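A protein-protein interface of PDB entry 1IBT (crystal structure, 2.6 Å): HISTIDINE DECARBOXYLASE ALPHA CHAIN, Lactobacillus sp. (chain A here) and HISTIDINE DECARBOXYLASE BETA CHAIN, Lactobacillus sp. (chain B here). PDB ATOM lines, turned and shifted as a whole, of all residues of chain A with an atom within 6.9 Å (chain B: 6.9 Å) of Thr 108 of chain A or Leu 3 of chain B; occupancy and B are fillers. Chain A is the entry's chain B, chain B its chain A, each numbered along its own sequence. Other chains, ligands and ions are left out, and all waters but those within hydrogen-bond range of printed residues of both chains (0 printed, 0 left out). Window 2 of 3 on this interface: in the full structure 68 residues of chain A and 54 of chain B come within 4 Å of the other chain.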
ATOM      1  N   VAL A   5     -34.099  17.642   0.576  1.00  0.00           N
ATOM      2  CA  VAL A   5     -32.822  17.107   0.181  1.00  0.00           C
ATOM      3  C   VAL A   5     -32.107  17.947  -0.847  1.00  0.00           C
ATOM      4  O   VAL A   5     -30.900  17.831  -0.984  1.00  0.00           O
ATOM      5  CB  VAL A   5     -33.001  15.675  -0.347  1.00  0.00           C
ATOM      6  CG1 VAL A   5     -33.516  14.878   0.815  1.00  0.00           C
ATOM      7  CG2 VAL A   5     -34.002  15.509  -1.442  1.00  0.00           C
ATOM      8  N   GLY A   7     -31.831  21.338  -0.829  1.00  0.00           N
ATOM      9  CA  GLY A   7     -31.679  22.747  -0.547  1.00  0.00           C
ATOM     10  C   GLY A   7     -30.749  23.173   0.527  1.00  0.00           C
ATOM     11  O   GLY A   7     -30.320  22.384   1.350  1.00  0.00           O
ATOM     12  N   ASP A  13     -26.926  27.426   6.154  1.00  0.00           N
ATOM     13  CA  ASP A  13     -26.163  26.383   5.486  1.00  0.00           C
ATOM     14  C   ASP A  13     -25.062  26.995   4.629  1.00  0.00           C
ATOM     15  O   ASP A  13     -23.983  26.431   4.489  1.00  0.00           O
ATOM     16  CB  ASP A  13     -27.010  25.559   4.554  1.00  0.00           C
ATOM     17  CG  ASP A  13     -27.994  24.563   5.134  1.00  0.00           C
ATOM     18  OD1 ASP A  13     -29.196  24.829   5.058  1.00  0.00           O
ATOM     19  OD2 ASP A  13     -27.589  23.483   5.566  1.00  0.00           O
ATOM     20  N   ALA A 104     -34.720  20.310   9.606  1.00  0.00           N
ATOM     21  CA  ALA A 104     -34.931  18.914   9.937  1.00  0.00           C
ATOM     22  C   ALA A 104     -33.694  18.339  10.621  1.00  0.00           C
ATOM     23  O   ALA A 104     -32.546  18.732  10.377  1.00  0.00           O
ATOM     24  CB  ALA A 104     -35.224  18.101   8.688  1.00  0.00           C
ATOM     25  N   LYS A 105     -33.958  17.415  11.528  1.00  0.00           N
ATOM     26  CA  LYS A 105     -32.896  16.799  12.300  1.00  0.00           C
ATOM     27  C   LYS A 105     -32.117  15.868  11.367  1.00  0.00           C
ATOM     28  O   LYS A 105     -30.888  15.836  11.397  1.00  0.00           O
ATOM     29  CB  LYS A 105     -33.565  16.045  13.458  1.00  0.00           C
ATOM     30  CG  LYS A 105     -32.816  15.154  14.444  1.00  0.00           C
ATOM     31  CD  LYS A 105     -33.816  14.054  14.859  1.00  0.00           C
ATOM     32  CE  LYS A 105     -34.242  13.180  13.646  1.00  0.00           C
ATOM     33  NZ  LYS A 105     -35.541  12.517  13.795  1.00  0.00           N
ATOM     34  N   ASP A 106     -32.832  15.109  10.537  1.00  0.00           N
ATOM     35  CA  ASP A 106     -32.206  14.221   9.586  1.00  0.00           C
ATOM     36  C   ASP A 106     -32.493  14.661   8.141  1.00  0.00           C
ATOM     37  O   ASP A 106     -33.443  14.161   7.519  1.00  0.00           O
ATOM     38  CB  ASP A 106     -32.726  12.801   9.860  1.00  0.00           C
ATOM     39  CG  ASP A 106     -32.165  11.662   8.980  1.00  0.00           C
ATOM     40  OD1 ASP A 106     -31.346  11.907   8.067  1.00  0.00           O
ATOM     41  OD2 ASP A 106     -32.588  10.514   9.196  1.00  0.00           O
ATOM     42  N   PRO A 107     -31.776  15.564   7.470  1.00  0.00           N
ATOM     43  CA  PRO A 107     -32.137  16.112   6.167  1.00  0.00           C
ATOM     44  C   PRO A 107     -32.069  15.076   5.064  1.00  0.00           C
ATOM     45  O   PRO A 107     -32.233  15.359   3.884  1.00  0.00           O
ATOM     46  CB  PRO A 107     -31.189  17.242   5.923  1.00  0.00           C
ATOM     47  CG  PRO A 107     -30.692  17.595   7.293  1.00  0.00           C
ATOM     48  CD  PRO A 107     -30.611  16.242   7.975  1.00  0.00           C
ATOM     49  N   THR A 108     -31.794  13.846   5.408  1.00  0.00           N
ATOM     50  CA  THR A 108     -31.754  12.791   4.453  1.00  0.00           C
ATOM     51  C   THR A 108     -33.110  12.150   4.420  1.00  0.00           C
ATOM     52  O   THR A 108     -33.565  11.714   3.377  1.00  0.00           O
ATOM     53  CB  THR A 108     -30.619  11.918   4.953  1.00  0.00           C
ATOM     54  OG1 THR A 108     -29.467  12.780   4.819  1.00  0.00           O
ATOM     55  CG2 THR A 108     -30.535  10.543   4.279  1.00  0.00           C
ATOM     56  N   LYS A 109     -33.765  12.041   5.552  1.00  0.00           N
ATOM     57  CA  LYS A 109     -35.067  11.414   5.593  1.00  0.00           C
ATOM     58  C   LYS A 109     -36.171  12.459   5.525  1.00  0.00           C
ATOM     59  O   LYS A 109     -37.170  12.255   4.835  1.00  0.00           O
ATOM     60  CB  LYS A 109     -35.102  10.583   6.885  1.00  0.00           C
ATOM     61  CG  LYS A 109     -36.417   9.974   7.389  1.00  0.00           C
ATOM     62  CD  LYS A 109     -36.309   9.716   8.925  1.00  0.00           C
ATOM     63  CE  LYS A 109     -37.651   9.571   9.653  1.00  0.00           C
ATOM     64  NZ  LYS A 109     -38.376  10.837   9.647  1.00  0.00           N
ATOM     65  N   ASP A 110     -35.979  13.604   6.189  1.00  0.00           N
ATOM     66  CA  ASP A 110     -37.023  14.605   6.383  1.00  0.00           C
ATOM     67  C   ASP A 110     -36.696  15.969   5.813  1.00  0.00           C
ATOM     68  O   ASP A 110     -35.525  16.383   5.765  1.00  0.00           O
ATOM     69  CB  ASP A 110     -37.311  14.826   7.870  1.00  0.00           C
ATOM     70  CG  ASP A 110     -37.792  13.611   8.616  1.00  0.00           C
ATOM     71  OD1 ASP A 110     -38.697  12.889   8.159  1.00  0.00           O
ATOM     72  OD2 ASP A 110     -37.248  13.343   9.693  1.00  0.00           O
ATOM     73  N   SER A 111     -37.744  16.720   5.459  1.00  0.00           N
ATOM     74  CA  SER A 111     -37.578  18.057   4.950  1.00  0.00           C
ATOM     75  C   SER A 111     -37.627  19.093   6.051  1.00  0.00           C
ATOM     76  O   SER A 111     -38.246  18.925   7.099  1.00  0.00           O
ATOM     77  CB  SER A 111     -38.654  18.334   3.957  1.00  0.00           C
ATOM     78  OG  SER A 111     -38.418  19.559   3.269  1.00  0.00           O
ATOM     79  N   GLU A 205     -20.625  27.184   1.270  1.00  0.00           N
ATOM     80  CA  GLU A 205     -20.920  26.666   2.579  1.00  0.00           C
ATOM     81  C   GLU A 205     -19.731  26.643   3.522  1.00  0.00           C
ATOM     82  O   GLU A 205     -19.865  26.301   4.710  1.00  0.00           O
ATOM     83  CB  GLU A 205     -21.526  25.275   2.506  1.00  0.00           C
ATOM     84  CG  GLU A 205     -21.034  24.206   1.633  1.00  0.00           C
ATOM     85  CD  GLU A 205     -21.649  22.841   1.906  1.00  0.00           C
ATOM     86  OE1 GLU A 205     -20.997  21.827   1.706  1.00  0.00           O
ATOM     87  OE2 GLU A 205     -22.803  22.669   2.263  1.00  0.00           O
ATOM     88  N   SER B   1     -20.618  19.362   2.002  1.00  0.00           N
ATOM     89  CA  SER B   1     -20.387  19.007   3.366  1.00  0.00           C
ATOM     90  C   SER B   1     -20.675  17.534   3.460  1.00  0.00           C
ATOM     91  O   SER B   1     -21.190  16.931   2.524  1.00  0.00           O
ATOM     92  CB  SER B   1     -21.328  19.770   4.299  1.00  0.00           C
ATOM     93  OG  SER B   1     -22.636  19.826   3.782  1.00  0.00           O
ATOM     94  N   GLU B   2     -20.401  16.922   4.588  1.00  0.00           N
ATOM     95  CA  GLU B   2     -20.544  15.489   4.727  1.00  0.00           C
ATOM     96  C   GLU B   2     -21.965  14.983   4.431  1.00  0.00           C
ATOM     97  O   GLU B   2     -22.223  13.844   4.021  1.00  0.00           O
ATOM     98  CB  GLU B   2     -20.013  15.275   6.142  1.00  0.00           C
ATOM     99  CG  GLU B   2     -19.208  14.003   6.467  1.00  0.00           C
ATOM    100  CD  GLU B   2     -20.107  12.855   6.947  1.00  0.00           C
ATOM    101  OE1 GLU B   2     -21.030  13.097   7.766  1.00  0.00           O
ATOM    102  OE2 GLU B   2     -19.963  11.709   6.476  1.00  0.00           O
ATOM    103  N   LEU B   3     -22.943  15.884   4.565  1.00  0.00           N
ATOM    104  CA  LEU B   3     -24.338  15.555   4.286  1.00  0.00           C
ATOM    105  C   LEU B   3     -24.540  15.375   2.778  1.00  0.00           C
ATOM    106  O   LEU B   3     -25.267  14.449   2.355  1.00  0.00           O
ATOM    107  CB  LEU B   3     -25.244  16.670   4.801  1.00  0.00           C
ATOM    108  CG  LEU B   3     -26.709  16.638   4.364  1.00  0.00           C
ATOM    109  CD1 LEU B   3     -27.403  15.442   4.989  1.00  0.00           C
ATOM    110  CD2 LEU B   3     -27.370  17.960   4.721  1.00  0.00           C
ATOM    111  N   ASP B   4     -23.890  16.222   1.959  1.00  0.00           N
ATOM    112  CA  ASP B   4     -24.007  16.104   0.521  1.00  0.00           C
ATOM    113  C   ASP B   4     -23.544  14.731   0.072  1.00  0.00           C
ATOM    114  O   ASP B   4     -24.215  14.048  -0.699  1.00  0.00           O
ATOM    115  CB  ASP B   4     -23.175  17.144  -0.137  1.00  0.00           C
ATOM    116  CG  ASP B   4     -23.713  18.494   0.202  1.00  0.00           C
ATOM    117  OD1 ASP B   4     -24.629  18.958  -0.439  1.00  0.00           O
ATOM    118  OD2 ASP B   4     -23.237  19.134   1.121  1.00  0.00           O
ATOM    119  N   ALA B   5     -22.447  14.252   0.652  1.00  0.00           N
ATOM    120  CA  ALA B   5     -21.977  12.913   0.376  1.00  0.00           C
ATOM    121  C   ALA B   5     -23.031  11.846   0.701  1.00  0.00           C
ATOM    122  O   ALA B   5     -23.127  10.865  -0.036  1.00  0.00           O
ATOM    123  CB  ALA B   5     -20.713  12.667   1.192  1.00  0.00           C
ATOM    124  N   LYS B   6     -23.869  11.949   1.741  1.00  0.00           N
ATOM    125  CA  LYS B   6     -24.910  10.953   2.014  1.00  0.00           C
ATOM    126  C   LYS B   6     -25.997  11.064   0.983  1.00  0.00           C
ATOM    127  O   LYS B   6     -26.564  10.064   0.548  1.00  0.00           O
ATOM    128  CB  LYS B   6     -25.550  11.144   3.407  1.00  0.00           C
ATOM    129  CG  LYS B   6     -24.523  10.900   4.499  1.00  0.00           C
ATOM    130  CD  LYS B   6     -25.032  10.959   5.949  1.00  0.00           C
ATOM    131  CE  LYS B   6     -23.906  10.511   6.938  1.00  0.00           C
ATOM    132  NZ  LYS B   6     -22.670  11.287   6.857  1.00  0.00           N
ATOM    133  N   LEU B   7     -26.202  12.306   0.557  1.00  0.00           N
ATOM    134  CA  LEU B   7     -27.239  12.659  -0.402  1.00  0.00           C
ATOM    135  C   LEU B   7     -27.016  12.149  -1.809  1.00  0.00           C
ATOM    136  O   LEU B   7     -27.879  11.593  -2.499  1.00  0.00           O
ATOM    137  CB  LEU B   7     -27.366  14.178  -0.413  1.00  0.00           C
ATOM    138  CG  LEU B   7     -28.451  14.944   0.326  1.00  0.00           C
ATOM    139  CD1 LEU B   7     -28.911  14.242   1.555  1.00  0.00           C
ATOM    140  CD2 LEU B   7     -27.874  16.294   0.692  1.00  0.00           C
ATOM    141  N   ASN B   8     -25.781  12.315  -2.234  1.00  0.00           N
ATOM    142  CA  ASN B   8     -25.352  11.934  -3.549  1.00  0.00           C
ATOM    143  C   ASN B   8     -25.560  10.464  -3.740  1.00  0.00           C
ATOM    144  O   ASN B   8     -25.931  10.064  -4.830  1.00  0.00           O
ATOM    145  CB  ASN B   8     -23.903  12.278  -3.744  1.00  0.00           C
ATOM    146  CG  ASN B   8     -23.640  13.761  -3.863  1.00  0.00           C
ATOM    147  OD1 ASN B   8     -22.563  14.237  -3.538  1.00  0.00           O
ATOM    148  ND2 ASN B   8     -24.551  14.593  -4.301  1.00  0.00           N
ATOM    149  N   LEU B  10     -28.041   8.862  -3.093  1.00  0.00           N
ATOM    150  CA  LEU B  10     -29.448   8.682  -3.392  1.00  0.00           C
ATOM    151  C   LEU B  10     -29.841   9.292  -4.716  1.00  0.00           C
ATOM    152  O   LEU B  10     -30.989   9.179  -5.153  1.00  0.00           O
ATOM    153  CB  LEU B  10     -30.280   9.329  -2.347  1.00  0.00           C
ATOM    154  CG  LEU B  10     -30.179   8.849  -0.941  1.00  0.00           C
ATOM    155  CD1 LEU B  10     -30.772   9.921  -0.067  1.00  0.00           C
ATOM    156  CD2 LEU B  10     -30.854   7.499  -0.782  1.00  0.00           C
ATOM    157  N   ARG B  14     -27.250  19.142  -4.399  1.00  0.00           N
ATOM    158  CA  ARG B  14     -27.767  20.409  -3.996  1.00  0.00           C
ATOM    159  C   ARG B  14     -26.974  21.448  -4.738  1.00  0.00           C
ATOM    160  O   ARG B  14     -26.550  22.449  -4.155  1.00  0.00           O
ATOM    161  CB  ARG B  14     -27.614  20.597  -2.471  1.00  0.00           C
ATOM    162  CG  ARG B  14     -28.323  19.557  -1.606  1.00  0.00           C
ATOM    163  CD  ARG B  14     -28.423  19.955  -0.137  1.00  0.00           C
ATOM    164  NE  ARG B  14     -27.129  19.941   0.535  1.00  0.00           N
ATOM    165  CZ  ARG B  14     -26.890  20.509   1.722  1.00  0.00           C
ATOM    166  NH1 ARG B  14     -27.888  21.131   2.376  1.00  0.00           N
ATOM    167  NH2 ARG B  14     -25.635  20.524   2.203  1.00  0.00           N
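N of Ser 1 of chain B sits at hydrogen-bond distance from OE1 of Glu 205 of chain A, at 2.5 Å.
NH1 of Arg 14 of chain B sits at hydrogen-bond distance from O of Gly 7 of chain A (2.9 Å).
NH1 of Arg 14 of chain B is in salt-bridge range of OD2 of Asp 13 of chain A.
The guanidinium group of Arg 14 of chain B lies within salt-bridge range of the side-chain carboxylate of Glu 205 of chain A, 3.6 Å away.
Printed residues of chain A that touch a printed residue of chain B: Val 5, Gly 7, Asp 13, Thr 108 and Glu 205.
Of the 10 printed residues of chain B, 5 touch a printed residue of chain A.
Among the printed residues, 9 pairs touch across the chains.
Among the printed residues, pairs that only touch across the chains: Val 5 of chain A with Arg 14 of chain B (3.2 Å), Thr 108 of chain A with Leu 3 of chain B (3.4 Å), Glu 205 of chain A with Asp 4 of chain B (3.6 Å), Thr 108 of chain A with Leu 7 of chain B (3.6 Å) and Val 5 of chain A with Leu 7 of chain B (3.8 Å).
Thr 108 of chain A touches two residues of chain B.
Leu 3 of chain B touches just one residue of chain A: Thr 108.
Printed residues of chain A within 4 Å of Leu 7 of chain B: Val 5 and Thr 108.
Printed residues of chain A within 4 Å of Asp 4 of chain B: Glu 205 (3.6 Å).
Lys 109 of chain A touches none of the printed residues of chain B.
The nearest residue of chain B that does not touch Thr 108 of chain A is Leu 10 of chain B (4.4 Å).
N of Ser 1 of chain B lies within hydrogen-bond range of OD2 of Asp 4 of chain B (2.8 Å).
OG of Ser 1 of chain B is in hydrogen-bond range of NH2 of Arg 14 of chain B, at 3.5 Å.
O of Asp 4 of chain B lies close to OD1 of Asn 8 of chain B, at 3.3 Å.
The side-chain carboxylate (OD1) of Asp 4 of chain B lies within salt-bridge range of the guanidinium group (NE) of Arg 14 of chain B (2.9 Å).
The backbone NH (N) of Thr 108 of chain A sits close to the side-chain carboxylate (OD1) of Asp 106 of chain A (3.3 Å).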
